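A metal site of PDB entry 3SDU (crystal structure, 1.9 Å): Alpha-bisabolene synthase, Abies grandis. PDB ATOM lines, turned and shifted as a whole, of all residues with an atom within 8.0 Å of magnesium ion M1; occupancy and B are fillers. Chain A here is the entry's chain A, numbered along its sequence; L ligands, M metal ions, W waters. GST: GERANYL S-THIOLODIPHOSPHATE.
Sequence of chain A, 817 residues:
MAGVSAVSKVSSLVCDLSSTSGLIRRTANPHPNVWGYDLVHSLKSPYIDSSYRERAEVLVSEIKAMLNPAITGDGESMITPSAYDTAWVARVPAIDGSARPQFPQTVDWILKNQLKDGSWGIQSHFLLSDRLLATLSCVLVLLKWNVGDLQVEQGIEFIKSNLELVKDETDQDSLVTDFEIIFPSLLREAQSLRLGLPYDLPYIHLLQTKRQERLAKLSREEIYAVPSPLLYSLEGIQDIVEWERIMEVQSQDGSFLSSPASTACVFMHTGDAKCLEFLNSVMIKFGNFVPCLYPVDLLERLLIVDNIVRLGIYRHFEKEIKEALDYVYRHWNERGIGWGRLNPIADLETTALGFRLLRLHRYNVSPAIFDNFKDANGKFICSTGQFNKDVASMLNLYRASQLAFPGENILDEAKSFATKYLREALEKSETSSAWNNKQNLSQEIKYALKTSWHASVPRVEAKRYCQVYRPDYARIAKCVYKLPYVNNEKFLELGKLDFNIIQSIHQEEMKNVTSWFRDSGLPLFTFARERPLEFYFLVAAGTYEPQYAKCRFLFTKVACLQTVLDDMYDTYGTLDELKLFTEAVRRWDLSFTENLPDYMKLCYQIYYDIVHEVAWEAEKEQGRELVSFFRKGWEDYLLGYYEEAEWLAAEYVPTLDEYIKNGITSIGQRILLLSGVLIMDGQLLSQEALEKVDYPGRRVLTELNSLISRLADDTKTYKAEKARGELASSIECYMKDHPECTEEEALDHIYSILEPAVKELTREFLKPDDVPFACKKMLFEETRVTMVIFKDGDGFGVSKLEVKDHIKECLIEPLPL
An oxygen (O1A) of the ligand is in salt-bridge range of the guanidinium group (NH1) of Arg 710 (2.8 Å).
Water W3 lies within hydrogen-bond range of OD2 of Asp 713 (2.8 Å) and O2B of the ligand (2.9 Å). Water W2 bridges the side-chain carboxylate (OE1) of Glu 721 (2.6 Å) and the side-chain carboxylate (OD1) of Asp 714 (2.7 Å). Water W1 lies within hydrogen-bond range of an oxygen (O1A) of the ligand (2.7 Å) and the guanidinium group (NH2) of Arg 710 (3.1 Å).
The side-chain carboxylate (OD1) of Asp 713 sits close to the guanidinium group (NH2) of Arg 710 (2.8 Å). The guanidinium group (NH2) of Arg 710 is in salt-bridge range of the side-chain carboxylate (OD1) of Asp 714. The backbone carbonyl oxygen (O) of Glu 721 sits at hydrogen-bond distance from the backbone NH (N) of Glu 726. O of Gly 795 is in hydrogen-bond range of N of Thr 717 (3.3 Å). OH of Tyr 659 is in hydrogen-bond range of NE of Arg 710.
Residues that only touch magnesium ion M1: Arg 710. Four residues have an atom within 4 Å of magnesium ion M1: Arg 710, Asp 713, Thr 717 and Glu 721.
Magnesium ion M1 is bound by the side-chain carboxylate of Glu 721 (2.1 Å), water W3 (2.1 Å), water W1 (2.1 Å), water W2 (2.1 Å), the side-chain carboxylate of Asp 713 (2.1 Å) and the side-chain hydroxyl of Thr 717 (2.2 Å). Magnesium ion M1 has six donor atoms within binding distance.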
ATOM      1  N   TYR A 659      30.027  18.931  20.508  1.00  0.00           N
ATOM      2  CA  TYR A 659      29.150  17.898  21.031  1.00  0.00           C
ATOM      3  C   TYR A 659      29.463  17.588  22.482  1.00  0.00           C
ATOM      4  O   TYR A 659      28.562  17.449  23.321  1.00  0.00           O
ATOM      5  CB  TYR A 659      29.276  16.626  20.197  1.00  0.00           C
ATOM      6  CG  TYR A 659      28.479  15.455  20.736  1.00  0.00           C
ATOM      7  CD1 TYR A 659      27.150  15.274  20.376  1.00  0.00           C
ATOM      8  CD2 TYR A 659      29.061  14.531  21.586  1.00  0.00           C
ATOM      9  CE1 TYR A 659      26.419  14.197  20.864  1.00  0.00           C
ATOM     10  CE2 TYR A 659      28.331  13.461  22.086  1.00  0.00           C
ATOM     11  CZ  TYR A 659      27.015  13.292  21.709  1.00  0.00           C
ATOM     12  OH  TYR A 659      26.307  12.227  22.213  1.00  0.00           O
ATOM     13  N   ILE A 667      23.823  16.442  29.672  1.00  0.00           N
ATOM     14  CA  ILE A 667      23.598  15.051  30.086  1.00  0.00           C
ATOM     15  C   ILE A 667      22.833  15.030  31.426  1.00  0.00           C
ATOM     16  O   ILE A 667      22.032  14.129  31.680  1.00  0.00           O
ATOM     17  CB  ILE A 667      24.927  14.242  30.156  1.00  0.00           C
ATOM     18  CG1 ILE A 667      24.657  12.746  30.372  1.00  0.00           C
ATOM     19  CG2 ILE A 667      25.845  14.766  31.252  1.00  0.00           C
ATOM     20  CD1 ILE A 667      23.915  12.087  29.242  1.00  0.00           C
ATOM     21  N   SER A 709      29.758   9.677  31.553  1.00  0.00           N
ATOM     22  CA  SER A 709      28.386   9.257  31.324  1.00  0.00           C
ATOM     23  C   SER A 709      27.967   9.465  29.867  1.00  0.00           C
ATOM     24  O   SER A 709      27.389   8.572  29.257  1.00  0.00           O
ATOM     25  CB  SER A 709      27.406  10.019  32.225  1.00  0.00           C
ATOM     26  OG  SER A 709      27.649   9.744  33.604  1.00  0.00           O
ATOM     27  N   ARG A 710      28.232  10.653  29.345  1.00  0.00           N
ATOM     28  CA  ARG A 710      27.859  10.986  27.976  1.00  0.00           C
ATOM     29  C   ARG A 710      28.510  10.028  26.969  1.00  0.00           C
ATOM     30  O   ARG A 710      27.837   9.459  26.107  1.00  0.00           O
ATOM     31  CB  ARG A 710      28.238  12.443  27.659  1.00  0.00           C
ATOM     32  CG  ARG A 710      28.076  12.865  26.180  1.00  0.00           C
ATOM     33  CD  ARG A 710      26.619  12.961  25.761  1.00  0.00           C
ATOM     34  NE  ARG A 710      26.022  11.647  25.582  1.00  0.00           N
ATOM     35  CZ  ARG A 710      24.711  11.405  25.582  1.00  0.00           C
ATOM     36  NH1 ARG A 710      23.833  12.396  25.763  1.00  0.00           N
ATOM     37  NH2 ARG A 710      24.274  10.160  25.407  1.00  0.00           N
ATOM     38  N   LEU A 711      29.821   9.854  27.093  1.00  0.00           N
ATOM     39  CA  LEU A 711      30.558   9.048  26.122  1.00  0.00           C
ATOM     40  C   LEU A 711      30.310   7.560  26.333  1.00  0.00           C
ATOM     41  O   LEU A 711      30.216   6.808  25.366  1.00  0.00           O
ATOM     42  CB  LEU A 711      32.060   9.371  26.175  1.00  0.00           C
ATOM     43  CG  LEU A 711      32.437  10.805  25.789  1.00  0.00           C
ATOM     44  CD1 LEU A 711      33.948  10.978  25.805  1.00  0.00           C
ATOM     45  CD2 LEU A 711      31.851  11.195  24.421  1.00  0.00           C
ATOM     46  N   ALA A 712      30.217   7.139  27.586  1.00  0.00           N
ATOM     47  CA  ALA A 712      29.916   5.742  27.854  1.00  0.00           C
ATOM     48  C   ALA A 712      28.551   5.404  27.284  1.00  0.00           C
ATOM     49  O   ALA A 712      28.377   4.381  26.635  1.00  0.00           O
ATOM     50  CB  ALA A 712      29.983   5.444  29.343  1.00  0.00           C
ATOM     51  N   ASP A 713      27.571   6.276  27.518  1.00  0.00           N
ATOM     52  CA  ASP A 713      26.260   6.080  26.928  1.00  0.00           C
ATOM     53  C   ASP A 713      26.374   5.913  25.405  1.00  0.00           C
ATOM     54  O   ASP A 713      25.817   4.986  24.830  1.00  0.00           O
ATOM     55  CB  ASP A 713      25.308   7.228  27.255  1.00  0.00           C
ATOM     56  CG  ASP A 713      23.990   7.096  26.514  1.00  0.00           C
ATOM     57  OD1 ASP A 713      23.949   7.388  25.296  1.00  0.00           O
ATOM     58  OD2 ASP A 713      22.987   6.689  27.139  1.00  0.00           O
ATOM     59  N   ASP A 714      27.103   6.819  24.771  1.00  0.00           N
ATOM     60  CA  ASP A 714      27.288   6.753  23.323  1.00  0.00           C
ATOM     61  C   ASP A 714      27.847   5.396  22.879  1.00  0.00           C
ATOM     62  O   ASP A 714      27.355   4.791  21.925  1.00  0.00           O
ATOM     63  CB  ASP A 714      28.206   7.876  22.826  1.00  0.00           C
ATOM     64  CG  ASP A 714      27.516   9.235  22.831  1.00  0.00           C
ATOM     65  OD1 ASP A 714      26.289   9.278  23.078  1.00  0.00           O
ATOM     66  OD2 ASP A 714      28.200  10.254  22.593  1.00  0.00           O
ATOM     67  N   THR A 715      28.869   4.912  23.587  1.00  0.00           N
ATOM     68  CA  THR A 715      29.507   3.644  23.216  1.00  0.00           C
ATOM     69  C   THR A 715      28.529   2.483  23.323  1.00  0.00           C
ATOM     70  O   THR A 715      28.635   1.496  22.589  1.00  0.00           O
ATOM     71  CB  THR A 715      30.744   3.331  24.095  1.00  0.00           C
ATOM     72  OG1 THR A 715      30.329   3.143  25.453  1.00  0.00           O
ATOM     73  CG2 THR A 715      31.772   4.453  24.015  1.00  0.00           C
ATOM     74  N   LYS A 716      27.583   2.604  24.253  1.00  0.00           N
ATOM     75  CA  LYS A 716      26.609   1.539  24.509  1.00  0.00           C
ATOM     76  C   LYS A 716      25.406   1.586  23.567  1.00  0.00           C
ATOM     77  O   LYS A 716      24.755   0.559  23.350  1.00  0.00           O
ATOM     78  CB  LYS A 716      26.121   1.627  25.960  1.00  0.00           C
ATOM     79  CG  LYS A 716      25.328   0.416  26.448  1.00  0.00           C
ATOM     80  CD  LYS A 716      26.154  -0.859  26.376  1.00  0.00           C
ATOM     81  CE  LYS A 716      25.514  -2.005  27.157  1.00  0.00           C
ATOM     82  NZ  LYS A 716      26.267  -3.275  26.933  1.00  0.00           N
ATOM     83  N   THR A 717      25.093   2.760  23.018  1.00  0.00           N
ATOM     84  CA  THR A 717      23.797   2.961  22.363  1.00  0.00           C
ATOM     85  C   THR A 717      23.798   3.570  20.960  1.00  0.00           C
ATOM     86  O   THR A 717      22.750   3.601  20.301  1.00  0.00           O
ATOM     87  CB  THR A 717      22.862   3.825  23.242  1.00  0.00           C
ATOM     88  OG1 THR A 717      23.424   5.123  23.434  1.00  0.00           O
ATOM     89  CG2 THR A 717      22.636   3.169  24.608  1.00  0.00           C
ATOM     90  N   TYR A 718      24.935   4.056  20.484  1.00  0.00           N
ATOM     91  CA  TYR A 718      24.949   4.841  19.241  1.00  0.00           C
ATOM     92  C   TYR A 718      24.383   4.120  18.000  1.00  0.00           C
ATOM     93  O   TYR A 718      23.831   4.764  17.105  1.00  0.00           O
ATOM     94  CB  TYR A 718      26.335   5.422  18.951  1.00  0.00           C
ATOM     95  CG  TYR A 718      27.268   4.465  18.255  1.00  0.00           C
ATOM     96  CD1 TYR A 718      27.923   3.470  18.960  1.00  0.00           C
ATOM     97  CD2 TYR A 718      27.497   4.560  16.884  1.00  0.00           C
ATOM     98  CE1 TYR A 718      28.779   2.594  18.338  1.00  0.00           C
ATOM     99  CE2 TYR A 718      28.355   3.687  16.252  1.00  0.00           C
ATOM    100  CZ  TYR A 718      28.992   2.710  16.980  1.00  0.00           C
ATOM    101  OH  TYR A 718      29.847   1.827  16.346  1.00  0.00           O
ATOM    102  N   LYS A 719      24.517   2.792  17.941  1.00  0.00           N
ATOM    103  CA  LYS A 719      24.043   2.041  16.776  1.00  0.00           C
ATOM    104  C   LYS A 719      22.530   1.975  16.683  1.00  0.00           C
ATOM    105  O   LYS A 719      21.962   2.021  15.584  1.00  0.00           O
ATOM    106  CB  LYS A 719      24.618   0.629  16.745  1.00  0.00           C
ATOM    107  CG  LYS A 719      26.078   0.535  16.346  1.00  0.00           C
ATOM    108  CD  LYS A 719      26.483  -0.908  16.102  1.00  0.00           C
ATOM    109  CE  LYS A 719      27.990  -1.089  16.173  1.00  0.00           C
ATOM    110  NZ  LYS A 719      28.685  -0.236  15.179  1.00  0.00           N
ATOM    111  N   ALA A 720      21.867   1.859  17.824  1.00  0.00           N
ATOM    112  CA  ALA A 720      20.412   1.849  17.866  1.00  0.00           C
ATOM    113  C   ALA A 720      19.892   3.207  17.392  1.00  0.00           C
ATOM    114  O   ALA A 720      18.912   3.289  16.649  1.00  0.00           O
ATOM    115  CB  ALA A 720      19.917   1.549  19.271  1.00  0.00           C
ATOM    116  N   GLU A 721      20.580   4.264  17.818  1.00  0.00           N
ATOM    117  CA  GLU A 721      20.196   5.625  17.494  1.00  0.00           C
ATOM    118  C   GLU A 721      20.522   5.985  16.045  1.00  0.00           C
ATOM    119  O   GLU A 721      19.949   6.922  15.490  1.00  0.00           O
ATOM    120  CB  GLU A 721      20.888   6.599  18.449  1.00  0.00           C
ATOM    121  CG  GLU A 721      20.552   6.326  19.899  1.00  0.00           C
ATOM    122  CD  GLU A 721      21.605   6.827  20.858  1.00  0.00           C
ATOM    123  OE1 GLU A 721      22.590   7.457  20.401  1.00  0.00           O
ATOM    124  OE2 GLU A 721      21.450   6.571  22.063  1.00  0.00           O
ATOM    125  N   GLU A 726      18.387   9.002  14.385  1.00  0.00           N
ATOM    126  CA  GLU A 726      18.377   9.881  15.549  1.00  0.00           C
ATOM    127  C   GLU A 726      19.486  10.925  15.531  1.00  0.00           C
ATOM    128  O   GLU A 726      20.389  10.897  14.681  1.00  0.00           O
ATOM    129  CB  GLU A 726      18.442   9.047  16.830  1.00  0.00           C
ATOM    130  CG  GLU A 726      17.973   9.745  18.093  1.00  0.00           C
ATOM    131  CD  GLU A 726      18.069   8.855  19.322  1.00  0.00           C
ATOM    132  OE1 GLU A 726      17.292   7.886  19.417  1.00  0.00           O
ATOM    133  OE2 GLU A 726      18.931   9.128  20.182  1.00  0.00           O
ATOM    134  N   LEU A 727      19.416  11.852  16.492  1.00  0.00           N
ATOM    135  CA  LEU A 727      20.429  12.880  16.688  1.00  0.00           C
ATOM    136  C   LEU A 727      21.836  12.281  16.778  1.00  0.00           C
ATOM    137  O   LEU A 727      22.070  11.347  17.555  1.00  0.00           O
ATOM    138  CB  LEU A 727      20.102  13.700  17.936  1.00  0.00           C
ATOM    139  CG  LEU A 727      21.160  14.658  18.502  1.00  0.00           C
ATOM    140  CD1 LEU A 727      20.535  15.982  18.889  1.00  0.00           C
ATOM    141  CD2 LEU A 727      21.884  14.023  19.689  1.00  0.00           C
ATOM    142  N   SER A 729      25.546  11.168  17.547  1.00  0.00           N
ATOM    143  CA  SER A 729      26.289  10.932  18.774  1.00  0.00           C
ATOM    144  C   SER A 729      27.746  11.360  18.599  1.00  0.00           C
ATOM    145  O   SER A 729      28.140  11.880  17.550  1.00  0.00           O
ATOM    146  CB  SER A 729      26.251   9.444  19.122  1.00  0.00           C
ATOM    147  OG  SER A 729      26.968   8.685  18.151  1.00  0.00           O
ATOM    148  N   PHE A 790      26.390   1.106  31.366  1.00  0.00           N
ATOM    149  CA  PHE A 790      26.883   1.320  30.002  1.00  0.00           C
ATOM    150  C   PHE A 790      28.124   0.484  29.662  1.00  0.00           C
ATOM    151  O   PHE A 790      28.810   0.773  28.681  1.00  0.00           O
ATOM    152  CB  PHE A 790      27.188   2.795  29.795  1.00  0.00           C
ATOM    153  CG  PHE A 790      25.989   3.678  29.934  1.00  0.00           C
ATOM    154  CD1 PHE A 790      24.829   3.394  29.235  1.00  0.00           C
ATOM    155  CD2 PHE A 790      26.008   4.781  30.763  1.00  0.00           C
ATOM    156  CE1 PHE A 790      23.702   4.190  29.361  1.00  0.00           C
ATOM    157  CE2 PHE A 790      24.884   5.586  30.891  1.00  0.00           C
ATOM    158  CZ  PHE A 790      23.732   5.293  30.181  1.00  0.00           C
ATOM    159  N   GLY A 795      27.171  -1.889  20.112  1.00  0.00           N
ATOM    160  CA  GLY A 795      26.229  -1.126  19.327  1.00  0.00           C
ATOM    161  C   GLY A 795      25.486  -0.114  20.172  1.00  0.00           C
ATOM    162  O   GLY A 795      26.000   0.987  20.382  1.00  0.00           O
ATOM    163  N   GLY A 797      22.511  -0.829  22.480  1.00  0.00           N
ATOM    164  CA  GLY A 797      21.466  -0.674  23.480  1.00  0.00           C
ATOM    165  C   GLY A 797      21.856  -1.103  24.879  1.00  0.00           C
ATOM    166  O   GLY A 797      22.699  -1.985  25.063  1.00  0.00           O
ATOM    167  N   VAL A 798      21.242  -0.475  25.860  1.00  0.00           N
ATOM    168  CA  VAL A 798      21.357  -0.894  27.250  1.00  0.00           C
ATOM    169  C   VAL A 798      20.498  -2.142  27.463  1.00  0.00           C
ATOM    170  O   VAL A 798      19.402  -2.247  26.909  1.00  0.00           O
ATOM    171  CB  VAL A 798      20.886   0.206  28.210  1.00  0.00           C
ATOM    172  CG1 VAL A 798      20.702  -0.343  29.618  1.00  0.00           C
ATOM    173  CG2 VAL A 798      21.861   1.377  28.188  1.00  0.00           C
HETATM  174  PA  GST L   1      19.993  10.523  26.273  1.00  0.00           P
HETATM  175  O1A GST L   1      21.447  10.892  25.699  1.00  0.00           O
HETATM  176  O2A GST L   1      20.103  10.315  27.747  1.00  0.00           O
HETATM  177  O3A GST L   1      19.031  11.792  25.976  1.00  0.00           O
HETATM  178  O1B GST L   1      19.422   9.229  25.500  1.00  0.00           O
HETATM  179  PB  GST L   1      18.482   8.280  26.422  1.00  0.00           P
HETATM  180  O2B GST L   1      18.460   6.944  25.783  1.00  0.00           O
HETATM  181  O3B GST L   1      19.105   8.158  27.903  1.00  0.00           O
HETATM  182  S1  GST L   1      16.485   8.953  26.533  1.00  0.00           S
HETATM  183  C1  GST L   1      15.750   7.689  27.626  1.00  0.00           C
HETATM  184  C2  GST L   1      14.544   7.089  26.957  1.00  0.00           C
HETATM  185  C3  GST L   1      13.724   6.331  27.629  1.00  0.00           C
HETATM  186  C10 GST L   1      13.572   6.548  29.118  1.00  0.00           C
HETATM  187  C4  GST L   1      13.291   5.009  27.040  1.00  0.00           C
HETATM  188  C5  GST L   1      14.137   3.895  27.675  1.00  0.00           C
HETATM  189  C6  GST L   1      14.542   2.883  26.636  1.00  0.00           C
HETATM  190  C7  GST L   1      15.793   2.823  26.243  1.00  0.00           C
HETATM  191  C9  GST L   1      16.407   1.498  25.865  1.00  0.00           C
HETATM  192  C8  GST L   1      16.609   4.084  26.133  1.00  0.00           C
HETATM  193 MG    MG M   1      22.587   7.137  23.680  1.00  0.00          MG
HETATM  194 MG    MG M   2      17.147  11.442  25.438  1.00  0.00          MG
HETATM  195  O   HOH W   1      21.875   9.099  23.668  1.00  0.00           O
HETATM  196  O   HOH W   2      24.180   7.772  22.452  1.00  0.00           O
HETATM  197  O   HOH W   3      21.166   6.429  25.034  1.00  0.00           O
